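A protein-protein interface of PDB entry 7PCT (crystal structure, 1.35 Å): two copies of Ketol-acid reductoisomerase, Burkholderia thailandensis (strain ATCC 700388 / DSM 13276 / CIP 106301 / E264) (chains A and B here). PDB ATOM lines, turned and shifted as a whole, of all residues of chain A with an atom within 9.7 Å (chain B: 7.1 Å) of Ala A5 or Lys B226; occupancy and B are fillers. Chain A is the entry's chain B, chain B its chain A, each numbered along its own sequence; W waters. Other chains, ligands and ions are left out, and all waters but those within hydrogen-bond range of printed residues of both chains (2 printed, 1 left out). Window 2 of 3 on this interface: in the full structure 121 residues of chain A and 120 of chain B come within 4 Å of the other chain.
O of Ala B227 is in hydrogen-bond range of OH of Tyr A155 (3.3 Å).
The side-chain carboxylate (OD2) of Asp A8 lies within salt-bridge range of the side-chain amino group (NZ) of Lys B226, 2.9 Å away.
N of Asn B224 is in hydrogen-bond range of OE1 of Gln A191, 2.7 Å away.
O of Ala A5 is in hydrogen-bond range of NZ of Lys B226 (3.1 Å).
The guanidinium group (NE) of Arg A136 is in salt-bridge range of the side-chain carboxylate (OE2) of Glu B231 (2.8 Å).
The side-chain amide nitrogen (ND2) of Asn B224 sits at hydrogen-bond distance from the side-chain carboxylate (OD1) of Asp A8 (2.9 Å).
OH of Tyr A155 is in hydrogen-bond range of OE2 of Glu B231 (2.8 Å).
CB of Ala A5 touches NE2 of Gln B327 (3.95 Å).
Ile A10 touches Phe B332 (CD1 to CE1, 3.8 Å).
Pro A153 touches Phe B332.
CE of Met A185 touches OD1 of Asn B224 (3.7 Å).
CE of Met A185 touches CB of Ala B227, at 3.9 Å.
Leu A187 touches Asn B224.
Gln A191 touches Phe B223 (OE1 to CA, 3.4 Å).
Phe B223 touches Leu A195 (CE2 to N, 3.8 Å).
CB of Ala B227 touches CD2 of Leu A195 (3.5 Å).
CG of Leu A195 touches CG of Glu B231, 3.5 Å away.
N of Met A185 lies within hydrogen-bond range of O of Ala A154.
OD1 of Asn B224 is in hydrogen-bond range of N of Ala B227.
N of Arg A136 is in hydrogen-bond range of O of Pro A153 (2.9 Å).
The side-chain amide oxygen (OD1) of Asn B224 is in hydrogen-bond range of the backbone NH (N) of Lys B226 (3.0 Å).
The backbone carbonyl oxygen (O) of Phe B332 lies within hydrogen-bond range of the guanidinium group (NH1) of Arg B329.
Ala A5 touches just these residues of chain B: Lys B226 (3.1 Å) and Gln B327 (3.95 Å).
Of the printed residues of chain B, Asp A8 touches Asn B224 and Lys B226.
Of the printed residues of chain A, Phe B223 touches Gln A191 and Leu A195.
No residue of chain A comes within 4 Å of Pro B225.
Of the printed residues of chain A, Lys B226 touches Ala A5 (3.1 Å) and Asp A8 (2.9 Å).
Ala B227 touches just these residues of chain A: Tyr A155, Met A185 and Leu A195.
No residue of chain A comes within 4 Å of Ala B228.
The nearest printed residue of chain A that does not touch Lys B226 is Ile A10 (4.01 Å).
Water W2 lies within hydrogen-bond range of OD2 of Asp A8 (2.6 Å) and OD1 of Asn B224 (2.9 Å).
Water W1 lies within hydrogen-bond range of the side-chain carboxylate of Glu B231 and the backbone carbonyl oxygen of Arg A136.
Hydrophobic or aromatic side chains of chain B that line the printed part of chain A: Phe B223, Ala B227, Leu B230, Ala B331 and Phe B332.
Hydrophobic or aromatic side chains of chain A within 4 Å of the printed part of chain B: Ala A5, Ile A10, Pro A153, Tyr A155, Met A185, Leu A187 and Leu A195.
Along chain A the printed residues that touch a printed residue of chain B span positions 5 to 195.
Among the printed residues, 20 pairs touch across the chains.
Among the printed residues, Asp or Glu carboxylates within 4 Å of a Lys or Arg side-chain nitrogen of the other chain: Asp A8 with Lys B226 (2.9 Å) and Arg A136 with Glu B231 (2.8 Å).
No position is printed for both chains.
Of the 20 pairs that touch across the chains among the printed residues, none has its exchanged pair printed and touching as well.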
ATOM      1  N   MET A   4     -27.202  11.815 -37.986  1.00  0.00           N
ATOM      2  CA  MET A   4     -28.489  11.285 -37.442  1.00  0.00           C
ATOM      3  C   MET A   4     -28.237  10.665 -36.062  1.00  0.00           C
ATOM      4  O   MET A   4     -27.251   9.912 -35.912  1.00  0.00           O
ATOM      5  CB  MET A   4     -29.096  10.218 -38.364  1.00  0.00           C
ATOM      6  CG  MET A   4     -29.426  10.702 -39.768  1.00  0.00           C
ATOM      7  SD  MET A   4     -30.727  11.968 -39.846  1.00  0.00           S
ATOM      8  CE  MET A   4     -32.176  11.023 -39.374  1.00  0.00           C
ATOM      9  N   ALA A   5     -29.119  10.950 -35.100  1.00  0.00           N
ATOM     10  CA  ALA A   5     -29.023  10.502 -33.689  1.00  0.00           C
ATOM     11  C   ALA A   5     -28.890   8.973 -33.628  1.00  0.00           C
ATOM     12  O   ALA A   5     -28.123   8.480 -32.783  1.00  0.00           O
ATOM     13  CB  ALA A   5     -30.232  10.982 -32.926  1.00  0.00           C
ATOM     14  N   SER A   6     -29.586   8.261 -34.522  1.00  0.00           N
ATOM     15  CA  SER A   6     -29.678   6.775 -34.575  1.00  0.00           C
ATOM     16  C   SER A   6     -28.325   6.135 -34.921  1.00  0.00           C
ATOM     17  O   SER A   6     -28.186   4.923 -34.702  1.00  0.00           O
ATOM     18  CB  SER A   6     -30.749   6.344 -35.551  1.00  0.00           C
ATOM     19  OG  SER A   6     -30.556   6.946 -36.825  1.00  0.00           O
ATOM     20  N   ASN A   7     -27.367   6.898 -35.456  1.00  0.00           N
ATOM     21  CA  ASN A   7     -26.106   6.339 -36.023  1.00  0.00           C
ATOM     22  C   ASN A   7     -24.982   6.334 -34.979  1.00  0.00           C
ATOM     23  O   ASN A   7     -23.888   5.844 -35.303  1.00  0.00           O
ATOM     24  CB  ASN A   7     -25.702   7.073 -37.305  1.00  0.00           C
ATOM     25  CG  ASN A   7     -26.569   6.692 -38.489  1.00  0.00           C
ATOM     26  OD1 ASN A   7     -27.112   5.591 -38.539  1.00  0.00           O
ATOM     27  ND2 ASN A   7     -26.707   7.596 -39.445  1.00  0.00           N
ATOM     28  N   ASP A   8     -25.219   6.812 -33.756  1.00  0.00           N
ATOM     29  CA  ASP A   8     -24.142   6.861 -32.732  1.00  0.00           C
ATOM     30  C   ASP A   8     -23.865   5.456 -32.184  1.00  0.00           C
ATOM     31  O   ASP A   8     -24.837   4.704 -31.887  1.00  0.00           O
ATOM     32  CB  ASP A   8     -24.466   7.891 -31.653  1.00  0.00           C
ATOM     33  CG  ASP A   8     -24.398   9.308 -32.196  1.00  0.00           C
ATOM     34  OD1 ASP A   8     -23.435   9.591 -32.926  1.00  0.00           O
ATOM     35  OD2 ASP A   8     -25.310  10.106 -31.886  1.00  0.00           O
ATOM     36  N   LEU A   9     -22.576   5.121 -32.063  1.00  0.00           N
ATOM     37  CA  LEU A   9     -22.093   3.871 -31.415  1.00  0.00           C
ATOM     38  C   LEU A   9     -21.629   4.233 -29.998  1.00  0.00           C
ATOM     39  O   LEU A   9     -20.606   4.935 -29.860  1.00  0.00           O
ATOM     40  CB  LEU A   9     -20.962   3.232 -32.236  1.00  0.00           C
ATOM     41  CG  LEU A   9     -21.150   3.198 -33.754  1.00  0.00           C
ATOM     42  CD1 LEU A   9     -19.911   2.646 -34.440  1.00  0.00           C
ATOM     43  CD2 LEU A   9     -22.385   2.407 -34.146  1.00  0.00           C
ATOM     44  N   ILE A  10     -22.393   3.821 -28.986  1.00  0.00           N
ATOM     45  CA  ILE A  10     -22.129   4.160 -27.558  1.00  0.00           C
ATOM     46  C   ILE A  10     -22.036   2.862 -26.762  1.00  0.00           C
ATOM     47  O   ILE A  10     -23.001   2.076 -26.761  1.00  0.00           O
ATOM     48  CB  ILE A  10     -23.191   5.118 -26.993  1.00  0.00           C
ATOM     49  CG1 ILE A  10     -23.222   6.397 -27.833  1.00  0.00           C
ATOM     50  CG2 ILE A  10     -22.932   5.400 -25.516  1.00  0.00           C
ATOM     51  CD1 ILE A  10     -24.412   7.289 -27.599  1.00  0.00           C
ATOM     52  N   ARG A 136     -14.004  12.949 -21.117  1.00  0.00           N
ATOM     53  CA  ARG A 136     -14.678  14.272 -21.168  1.00  0.00           C
ATOM     54  C   ARG A 136     -14.726  14.878 -19.762  1.00  0.00           C
ATOM     55  O   ARG A 136     -15.707  15.548 -19.421  1.00  0.00           O
ATOM     56  CB  ARG A 136     -16.093  14.161 -21.739  1.00  0.00           C
ATOM     57  CG  ARG A 136     -16.238  13.320 -22.996  1.00  0.00           C
ATOM     58  CD  ARG A 136     -15.088  13.448 -23.973  1.00  0.00           C
ATOM     59  NE  ARG A 136     -14.797  14.797 -24.435  1.00  0.00           N
ATOM     60  CZ  ARG A 136     -13.745  15.110 -25.179  1.00  0.00           C
ATOM     61  NH1 ARG A 136     -12.848  14.185 -25.484  1.00  0.00           N
ATOM     62  NH2 ARG A 136     -13.580  16.345 -25.623  1.00  0.00           N
ATOM     63  N   PRO A 153     -18.100  10.325 -19.273  1.00  0.00           N
ATOM     64  CA  PRO A 153     -18.093   9.897 -20.669  1.00  0.00           C
ATOM     65  C   PRO A 153     -16.681   9.970 -21.268  1.00  0.00           C
ATOM     66  O   PRO A 153     -15.826  10.685 -20.757  1.00  0.00           O
ATOM     67  CB  PRO A 153     -19.005  10.911 -21.388  1.00  0.00           C
ATOM     68  CG  PRO A 153     -19.772  11.581 -20.265  1.00  0.00           C
ATOM     69  CD  PRO A 153     -18.812  11.603 -19.096  1.00  0.00           C
ATOM     70  N   ALA A 154     -16.486   9.275 -22.382  1.00  0.00           N
ATOM     71  CA  ALA A 154     -15.271   9.382 -23.209  1.00  0.00           C
ATOM     72  C   ALA A 154     -15.656   9.163 -24.669  1.00  0.00           C
ATOM     73  O   ALA A 154     -16.729   8.582 -24.929  1.00  0.00           O
ATOM     74  CB  ALA A 154     -14.237   8.387 -22.742  1.00  0.00           C
ATOM     75  N   TYR A 155     -14.830   9.674 -25.577  1.00  0.00           N
ATOM     76  CA  TYR A 155     -14.911   9.377 -27.030  1.00  0.00           C
ATOM     77  C   TYR A 155     -13.770   8.432 -27.381  1.00  0.00           C
ATOM     78  O   TYR A 155     -12.698   8.502 -26.758  1.00  0.00           O
ATOM     79  CB  TYR A 155     -14.840  10.652 -27.874  1.00  0.00           C
ATOM     80  CG  TYR A 155     -15.803  11.725 -27.447  1.00  0.00           C
ATOM     81  CD1 TYR A 155     -17.046  11.412 -26.921  1.00  0.00           C
ATOM     82  CD2 TYR A 155     -15.460  13.061 -27.553  1.00  0.00           C
ATOM     83  CE1 TYR A 155     -17.919  12.399 -26.499  1.00  0.00           C
ATOM     84  CE2 TYR A 155     -16.333  14.060 -27.146  1.00  0.00           C
ATOM     85  CZ  TYR A 155     -17.555  13.728 -26.594  1.00  0.00           C
ATOM     86  OH  TYR A 155     -18.412  14.698 -26.162  1.00  0.00           O
ATOM     87  N   VAL A 184     -19.140   5.348 -23.698  1.00  0.00           N
ATOM     88  CA  VAL A 184     -17.960   5.629 -24.552  1.00  0.00           C
ATOM     89  C   VAL A 184     -18.437   5.643 -25.997  1.00  0.00           C
ATOM     90  O   VAL A 184     -18.890   4.608 -26.499  1.00  0.00           O
ATOM     91  CB  VAL A 184     -16.846   4.605 -24.297  1.00  0.00           C
ATOM     92  CG1 VAL A 184     -15.660   4.830 -25.213  1.00  0.00           C
ATOM     93  CG2 VAL A 184     -16.376   4.631 -22.849  1.00  0.00           C
ATOM     94  N   MET A 185     -18.367   6.808 -26.626  1.00  0.00           N
ATOM     95  CA  MET A 185     -18.956   7.020 -27.966  1.00  0.00           C
ATOM     96  C   MET A 185     -17.864   7.060 -29.033  1.00  0.00           C
ATOM     97  O   MET A 185     -16.858   7.737 -28.842  1.00  0.00           O
ATOM     98  CB  MET A 185     -19.754   8.322 -28.000  1.00  0.00           C
ATOM     99  CG  MET A 185     -20.474   8.526 -29.313  1.00  0.00           C
ATOM    100  SD  MET A 185     -21.712   9.817 -29.285  1.00  0.00           S
ATOM    101  CE  MET A 185     -20.663  11.267 -29.311  1.00  0.00           C
ATOM    102  N   ALA A 186     -18.099   6.394 -30.157  1.00  0.00           N
ATOM    103  CA  ALA A 186     -17.203   6.493 -31.327  1.00  0.00           C
ATOM    104  C   ALA A 186     -17.215   7.932 -31.847  1.00  0.00           C
ATOM    105  O   ALA A 186     -18.291   8.473 -32.129  1.00  0.00           O
ATOM    106  CB  ALA A 186     -17.632   5.523 -32.388  1.00  0.00           C
ATOM    107  N   LEU A 187     -16.045   8.547 -31.947  1.00  0.00           N
ATOM    108  CA  LEU A 187     -15.896   9.889 -32.559  1.00  0.00           C
ATOM    109  C   LEU A 187     -14.494   9.983 -33.160  1.00  0.00           C
ATOM    110  O   LEU A 187     -13.527   9.628 -32.471  1.00  0.00           O
ATOM    111  CB  LEU A 187     -16.137  10.972 -31.501  1.00  0.00           C
ATOM    112  CG  LEU A 187     -16.393  12.368 -32.064  1.00  0.00           C
ATOM    113  CD1 LEU A 187     -17.828  12.515 -32.546  1.00  0.00           C
ATOM    114  CD2 LEU A 187     -16.068  13.452 -31.044  1.00  0.00           C
ATOM    115  N   GLN A 191     -12.242  15.168 -35.337  1.00  0.00           N
ATOM    116  CA  GLN A 191     -13.414  15.857 -34.748  1.00  0.00           C
ATOM    117  C   GLN A 191     -13.193  16.051 -33.239  1.00  0.00           C
ATOM    118  O   GLN A 191     -13.490  17.141 -32.714  1.00  0.00           O
ATOM    119  CB  GLN A 191     -14.713  15.101 -35.003  1.00  0.00           C
ATOM    120  CG  GLN A 191     -15.898  15.851 -34.415  1.00  0.00           C
ATOM    121  CD  GLN A 191     -17.267  15.280 -34.670  1.00  0.00           C
ATOM    122  OE1 GLN A 191     -18.247  15.802 -34.152  1.00  0.00           O
ATOM    123  NE2 GLN A 191     -17.345  14.214 -35.449  1.00  0.00           N
ATOM    124  N   LEU A 195     -13.311  19.821 -31.455  1.00  0.00           N
ATOM    125  CA  LEU A 195     -14.395  19.961 -30.451  1.00  0.00           C
ATOM    126  C   LEU A 195     -13.789  20.295 -29.077  1.00  0.00           C
ATOM    127  O   LEU A 195     -14.225  21.259 -28.422  1.00  0.00           O
ATOM    128  CB  LEU A 195     -15.177  18.649 -30.444  1.00  0.00           C
ATOM    129  CG  LEU A 195     -16.273  18.555 -29.402  1.00  0.00           C
ATOM    130  CD1 LEU A 195     -17.305  19.654 -29.613  1.00  0.00           C
ATOM    131  CD2 LEU A 195     -16.917  17.180 -29.436  1.00  0.00           C
ATOM    132  N   PHE B 215     -23.252  25.204 -28.422  1.00  0.00           N
ATOM    133  CA  PHE B 215     -23.948  24.041 -29.023  1.00  0.00           C
ATOM    134  C   PHE B 215     -24.368  24.371 -30.463  1.00  0.00           C
ATOM    135  O   PHE B 215     -24.086  23.583 -31.401  1.00  0.00           O
ATOM    136  CB  PHE B 215     -25.143  23.646 -28.161  1.00  0.00           C
ATOM    137  CG  PHE B 215     -25.986  22.574 -28.791  1.00  0.00           C
ATOM    138  CD1 PHE B 215     -25.568  21.254 -28.773  1.00  0.00           C
ATOM    139  CD2 PHE B 215     -27.196  22.886 -29.391  1.00  0.00           C
ATOM    140  CE1 PHE B 215     -26.335  20.265 -29.361  1.00  0.00           C
ATOM    141  CE2 PHE B 215     -27.958  21.893 -29.983  1.00  0.00           C
ATOM    142  CZ  PHE B 215     -27.530  20.587 -29.958  1.00  0.00           C
ATOM    143  N   VAL B 219     -23.009  22.584 -33.953  1.00  0.00           N
ATOM    144  CA  VAL B 219     -23.933  21.818 -34.832  1.00  0.00           C
ATOM    145  C   VAL B 219     -23.905  22.437 -36.239  1.00  0.00           C
ATOM    146  O   VAL B 219     -23.833  21.672 -37.245  1.00  0.00           O
ATOM    147  CB  VAL B 219     -25.342  21.737 -34.218  1.00  0.00           C
ATOM    148  CG1 VAL B 219     -26.357  21.190 -35.211  1.00  0.00           C
ATOM    149  CG2 VAL B 219     -25.334  20.891 -32.947  1.00  0.00           C
ATOM    150  N   PHE B 223     -20.465  19.351 -36.385  1.00  0.00           N
ATOM    151  CA  PHE B 223     -20.059  18.461 -35.272  1.00  0.00           C
ATOM    152  C   PHE B 223     -21.236  17.584 -34.837  1.00  0.00           C
ATOM    153  O   PHE B 223     -22.408  17.986 -34.934  1.00  0.00           O
ATOM    154  CB  PHE B 223     -19.509  19.273 -34.098  1.00  0.00           C
ATOM    155  CG  PHE B 223     -18.153  19.854 -34.400  1.00  0.00           C
ATOM    156  CD1 PHE B 223     -18.020  21.019 -35.142  1.00  0.00           C
ATOM    157  CD2 PHE B 223     -17.003  19.193 -33.994  1.00  0.00           C
ATOM    158  CE1 PHE B 223     -16.766  21.523 -35.448  1.00  0.00           C
ATOM    159  CE2 PHE B 223     -15.752  19.699 -34.300  1.00  0.00           C
ATOM    160  CZ  PHE B 223     -15.637  20.858 -35.028  1.00  0.00           C
ATOM    161  N   ASN B 224     -20.893  16.400 -34.341  1.00  0.00           N
ATOM    162  CA  ASN B 224     -21.838  15.436 -33.733  1.00  0.00           C
ATOM    163  C   ASN B 224     -22.647  16.137 -32.643  1.00  0.00           C
ATOM    164  O   ASN B 224     -22.074  16.652 -31.684  1.00  0.00           O
ATOM    165  CB  ASN B 224     -21.059  14.248 -33.179  1.00  0.00           C
ATOM    166  CG  ASN B 224     -21.962  13.169 -32.637  1.00  0.00           C
ATOM    167  OD1 ASN B 224     -22.654  13.383 -31.645  1.00  0.00           O
ATOM    168  ND2 ASN B 224     -21.947  12.011 -33.278  1.00  0.00           N
ATOM    169  N   PRO B 225     -23.991  16.242 -32.756  1.00  0.00           N
ATOM    170  CA  PRO B 225     -24.768  16.942 -31.734  1.00  0.00           C
ATOM    171  C   PRO B 225     -24.673  16.381 -30.307  1.00  0.00           C
ATOM    172  O   PRO B 225     -24.666  17.177 -29.370  1.00  0.00           O
ATOM    173  CB  PRO B 225     -26.212  16.878 -32.249  1.00  0.00           C
ATOM    174  CG  PRO B 225     -26.052  16.740 -33.754  1.00  0.00           C
ATOM    175  CD  PRO B 225     -24.817  15.873 -33.919  1.00  0.00           C
ATOM    176  N   LYS B 226     -24.572  15.062 -30.133  1.00  0.00           N
ATOM    177  CA  LYS B 226     -24.439  14.483 -28.773  1.00  0.00           C
ATOM    178  C   LYS B 226     -23.112  14.956 -28.180  1.00  0.00           C
ATOM    179  O   LYS B 226     -23.091  15.379 -27.012  1.00  0.00           O
ATOM    180  CB  LYS B 226     -24.484  12.958 -28.798  1.00  0.00           C
ATOM    181  CG  LYS B 226     -25.860  12.354 -28.992  1.00  0.00           C
ATOM    182  CD  LYS B 226     -25.841  10.874 -28.689  1.00  0.00           C
ATOM    183  CE  LYS B 226     -27.194  10.219 -28.822  1.00  0.00           C
ATOM    184  NZ  LYS B 226     -27.647  10.221 -30.231  1.00  0.00           N
ATOM    185  N   ALA B 227     -22.037  14.896 -28.969  1.00  0.00           N
ATOM    186  CA  ALA B 227     -20.711  15.342 -28.503  1.00  0.00           C
ATOM    187  C   ALA B 227     -20.749  16.844 -28.209  1.00  0.00           C
ATOM    188  O   ALA B 227     -20.200  17.271 -27.182  1.00  0.00           O
ATOM    189  CB  ALA B 227     -19.640  14.975 -29.498  1.00  0.00           C
ATOM    190  N   ALA B 228     -21.379  17.642 -29.071  1.00  0.00           N
ATOM    191  CA  ALA B 228     -21.473  19.100 -28.858  1.00  0.00           C
ATOM    192  C   ALA B 228     -22.172  19.360 -27.514  1.00  0.00           C
ATOM    193  O   ALA B 228     -21.661  20.182 -26.719  1.00  0.00           O
ATOM    194  CB  ALA B 228     -22.183  19.760 -30.006  1.00  0.00           C
ATOM    195  N   LEU B 229     -23.289  18.678 -27.249  1.00  0.00           N
ATOM    196  CA  LEU B 229     -24.094  18.862 -26.009  1.00  0.00           C
ATOM    197  C   LEU B 229     -23.215  18.479 -24.812  1.00  0.00           C
ATOM    198  O   LEU B 229     -23.156  19.219 -23.819  1.00  0.00           O
ATOM    199  CB  LEU B 229     -25.354  17.989 -26.114  1.00  0.00           C
ATOM    200  CG  LEU B 229     -26.516  18.213 -25.144  1.00  0.00           C
ATOM    201  CD1 LEU B 229     -26.157  17.902 -23.704  1.00  0.00           C
ATOM    202  CD2 LEU B 229     -27.100  19.602 -25.282  1.00  0.00           C
ATOM    203  N   LEU B 230     -22.529  17.343 -24.896  1.00  0.00           N
ATOM    204  CA  LEU B 230     -21.660  16.881 -23.791  1.00  0.00           C
ATOM    205  C   LEU B 230     -20.589  17.933 -23.499  1.00  0.00           C
ATOM    206  O   LEU B 230     -20.383  18.264 -22.322  1.00  0.00           O
ATOM    207  CB  LEU B 230     -21.022  15.540 -24.153  1.00  0.00           C
ATOM    208  CG  LEU B 230     -21.952  14.330 -24.035  1.00  0.00           C
ATOM    209  CD1 LEU B 230     -21.311  13.104 -24.656  1.00  0.00           C
ATOM    210  CD2 LEU B 230     -22.331  14.064 -22.585  1.00  0.00           C
ATOM    211  N   GLU B 231     -19.946  18.481 -24.525  1.00  0.00           N
ATOM    212  CA  GLU B 231     -18.822  19.410 -24.267  1.00  0.00           C
ATOM    213  C   GLU B 231     -19.355  20.699 -23.644  1.00  0.00           C
ATOM    214  O   GLU B 231     -18.692  21.236 -22.754  1.00  0.00           O
ATOM    215  CB  GLU B 231     -18.040  19.683 -25.542  1.00  0.00           C
ATOM    216  CG  GLU B 231     -17.366  18.445 -26.077  1.00  0.00           C
ATOM    217  CD  GLU B 231     -16.537  17.701 -25.052  1.00  0.00           C
ATOM    218  OE1 GLU B 231     -15.501  18.254 -24.641  1.00  0.00           O
ATOM    219  OE2 GLU B 231     -16.932  16.582 -24.659  1.00  0.00           O
ATOM    220  N   VAL B 232     -20.486  21.221 -24.113  1.00  0.00           N
ATOM    221  CA  VAL B 232     -20.887  22.585 -23.654  1.00  0.00           C
ATOM    222  C   VAL B 232     -21.465  22.520 -22.224  1.00  0.00           C
ATOM    223  O   VAL B 232     -21.367  23.532 -21.525  1.00  0.00           O
ATOM    224  CB  VAL B 232     -21.787  23.328 -24.656  1.00  0.00           C
ATOM    225  CG1 VAL B 232     -21.052  23.552 -25.971  1.00  0.00           C
ATOM    226  CG2 VAL B 232     -23.123  22.634 -24.884  1.00  0.00           C
ATOM    227  N   GLY B 234     -23.153  18.921 -20.939  1.00  0.00           N
ATOM    228  CA  GLY B 234     -23.762  17.610 -20.649  1.00  0.00           C
ATOM    229  C   GLY B 234     -22.822  16.612 -19.986  1.00  0.00           C
ATOM    230  O   GLY B 234     -23.324  15.703 -19.309  1.00  0.00           O
ATOM    231  N   ALA B 324     -31.781  17.751 -27.608  1.00  0.00           N
ATOM    232  CA  ALA B 324     -30.469  17.067 -27.553  1.00  0.00           C
ATOM    233  C   ALA B 324     -30.202  16.595 -26.123  1.00  0.00           C
ATOM    234  O   ALA B 324     -29.687  15.486 -25.941  1.00  0.00           O
ATOM    235  CB  ALA B 324     -29.386  17.991 -28.040  1.00  0.00           C
ATOM    236  N   GLN B 327     -31.857  13.277 -25.528  1.00  0.00           N
ATOM    237  CA  GLN B 327     -31.204  12.193 -26.306  1.00  0.00           C
ATOM    238  C   GLN B 327     -29.887  11.801 -25.634  1.00  0.00           C
ATOM    239  O   GLN B 327     -29.609  10.597 -25.496  1.00  0.00           O
ATOM    240  CB  GLN B 327     -30.943  12.638 -27.740  1.00  0.00           C
ATOM    241  CG  GLN B 327     -32.213  12.747 -28.564  1.00  0.00           C
ATOM    242  CD  GLN B 327     -31.956  13.366 -29.916  1.00  0.00           C
ATOM    243  OE1 GLN B 327     -30.975  14.081 -30.120  1.00  0.00           O
ATOM    244  NE2 GLN B 327     -32.849  13.102 -30.854  1.00  0.00           N
ATOM    245  N   VAL B 328     -29.098  12.787 -25.216  1.00  0.00           N
ATOM    246  CA  VAL B 328     -27.792  12.543 -24.548  1.00  0.00           C
ATOM    247  C   VAL B 328     -28.037  11.865 -23.200  1.00  0.00           C
ATOM    248  O   VAL B 328     -27.346  10.902 -22.893  1.00  0.00           O
ATOM    249  CB  VAL B 328     -26.998  13.844 -24.377  1.00  0.00           C
ATOM    250  CG1 VAL B 328     -25.844  13.644 -23.411  1.00  0.00           C
ATOM    251  CG2 VAL B 328     -26.519  14.352 -25.725  1.00  0.00           C
ATOM    252  N   ARG B 329     -28.996  12.343 -22.415  1.00  0.00           N
ATOM    253  CA  ARG B 329     -29.205  11.807 -21.052  1.00  0.00           C
ATOM    254  C   ARG B 329     -29.745  10.374 -21.124  1.00  0.00           C
ATOM    255  O   ARG B 329     -29.419   9.576 -20.227  1.00  0.00           O
ATOM    256  CB  ARG B 329     -30.111  12.729 -20.237  1.00  0.00           C
ATOM    257  CG  ARG B 329     -30.122  12.379 -18.759  1.00  0.00           C
ATOM    258  CD  ARG B 329     -28.724  12.250 -18.155  1.00  0.00           C
ATOM    259  NE  ARG B 329     -27.846  13.358 -18.498  1.00  0.00           N
ATOM    260  CZ  ARG B 329     -26.596  13.309 -18.992  1.00  0.00           C
ATOM    261  NH1 ARG B 329     -25.953  12.166 -19.199  1.00  0.00           N
ATOM    262  NH2 ARG B 329     -25.974  14.454 -19.254  1.00  0.00           N
ATOM    263  N   ALA B 330     -30.472  10.013 -22.181  1.00  0.00           N
ATOM    264  CA  ALA B 330     -30.927   8.619 -22.385  1.00  0.00           C
ATOM    265  C   ALA B 330     -29.737   7.749 -22.803  1.00  0.00           C
ATOM    266  O   ALA B 330     -29.785   6.530 -22.545  1.00  0.00           O
ATOM    267  CB  ALA B 330     -32.039   8.543 -23.395  1.00  0.00           C
ATOM    268  N   ALA B 331     -28.716   8.322 -23.442  1.00  0.00           N
ATOM    269  CA  ALA B 331     -27.592   7.554 -24.043  1.00  0.00           C
ATOM    270  C   ALA B 331     -26.392   7.454 -23.091  1.00  0.00           C
ATOM    271  O   ALA B 331     -25.590   6.498 -23.238  1.00  0.00           O
ATOM    272  CB  ALA B 331     -27.183   8.177 -25.353  1.00  0.00           C
ATOM    273  N   PHE B 332     -26.236   8.396 -22.167  1.00  0.00           N
ATOM    274  CA  PHE B 332     -25.089   8.453 -21.223  1.00  0.00           C
ATOM    275  C   PHE B 332     -25.622   8.531 -19.794  1.00  0.00           C
ATOM    276  O   PHE B 332     -26.489   9.381 -19.500  1.00  0.00           O
ATOM    277  CB  PHE B 332     -24.183   9.660 -21.492  1.00  0.00           C
ATOM    278  CG  PHE B 332     -23.499   9.644 -22.835  1.00  0.00           C
ATOM    279  CD1 PHE B 332     -24.143  10.124 -23.967  1.00  0.00           C
ATOM    280  CD2 PHE B 332     -22.217   9.134 -22.970  1.00  0.00           C
ATOM    281  CE1 PHE B 332     -23.514  10.098 -25.199  1.00  0.00           C
ATOM    282  CE2 PHE B 332     -21.585   9.117 -24.198  1.00  0.00           C
ATOM    283  CZ  PHE B 332     -22.237   9.600 -25.308  1.00  0.00           C
HETATM  284  O   HOH W   1     -16.609  17.731 -21.653  1.00  0.00           O
HETATM  285  O   HOH W   2     -25.253  12.559 -32.657  1.00  0.00           O
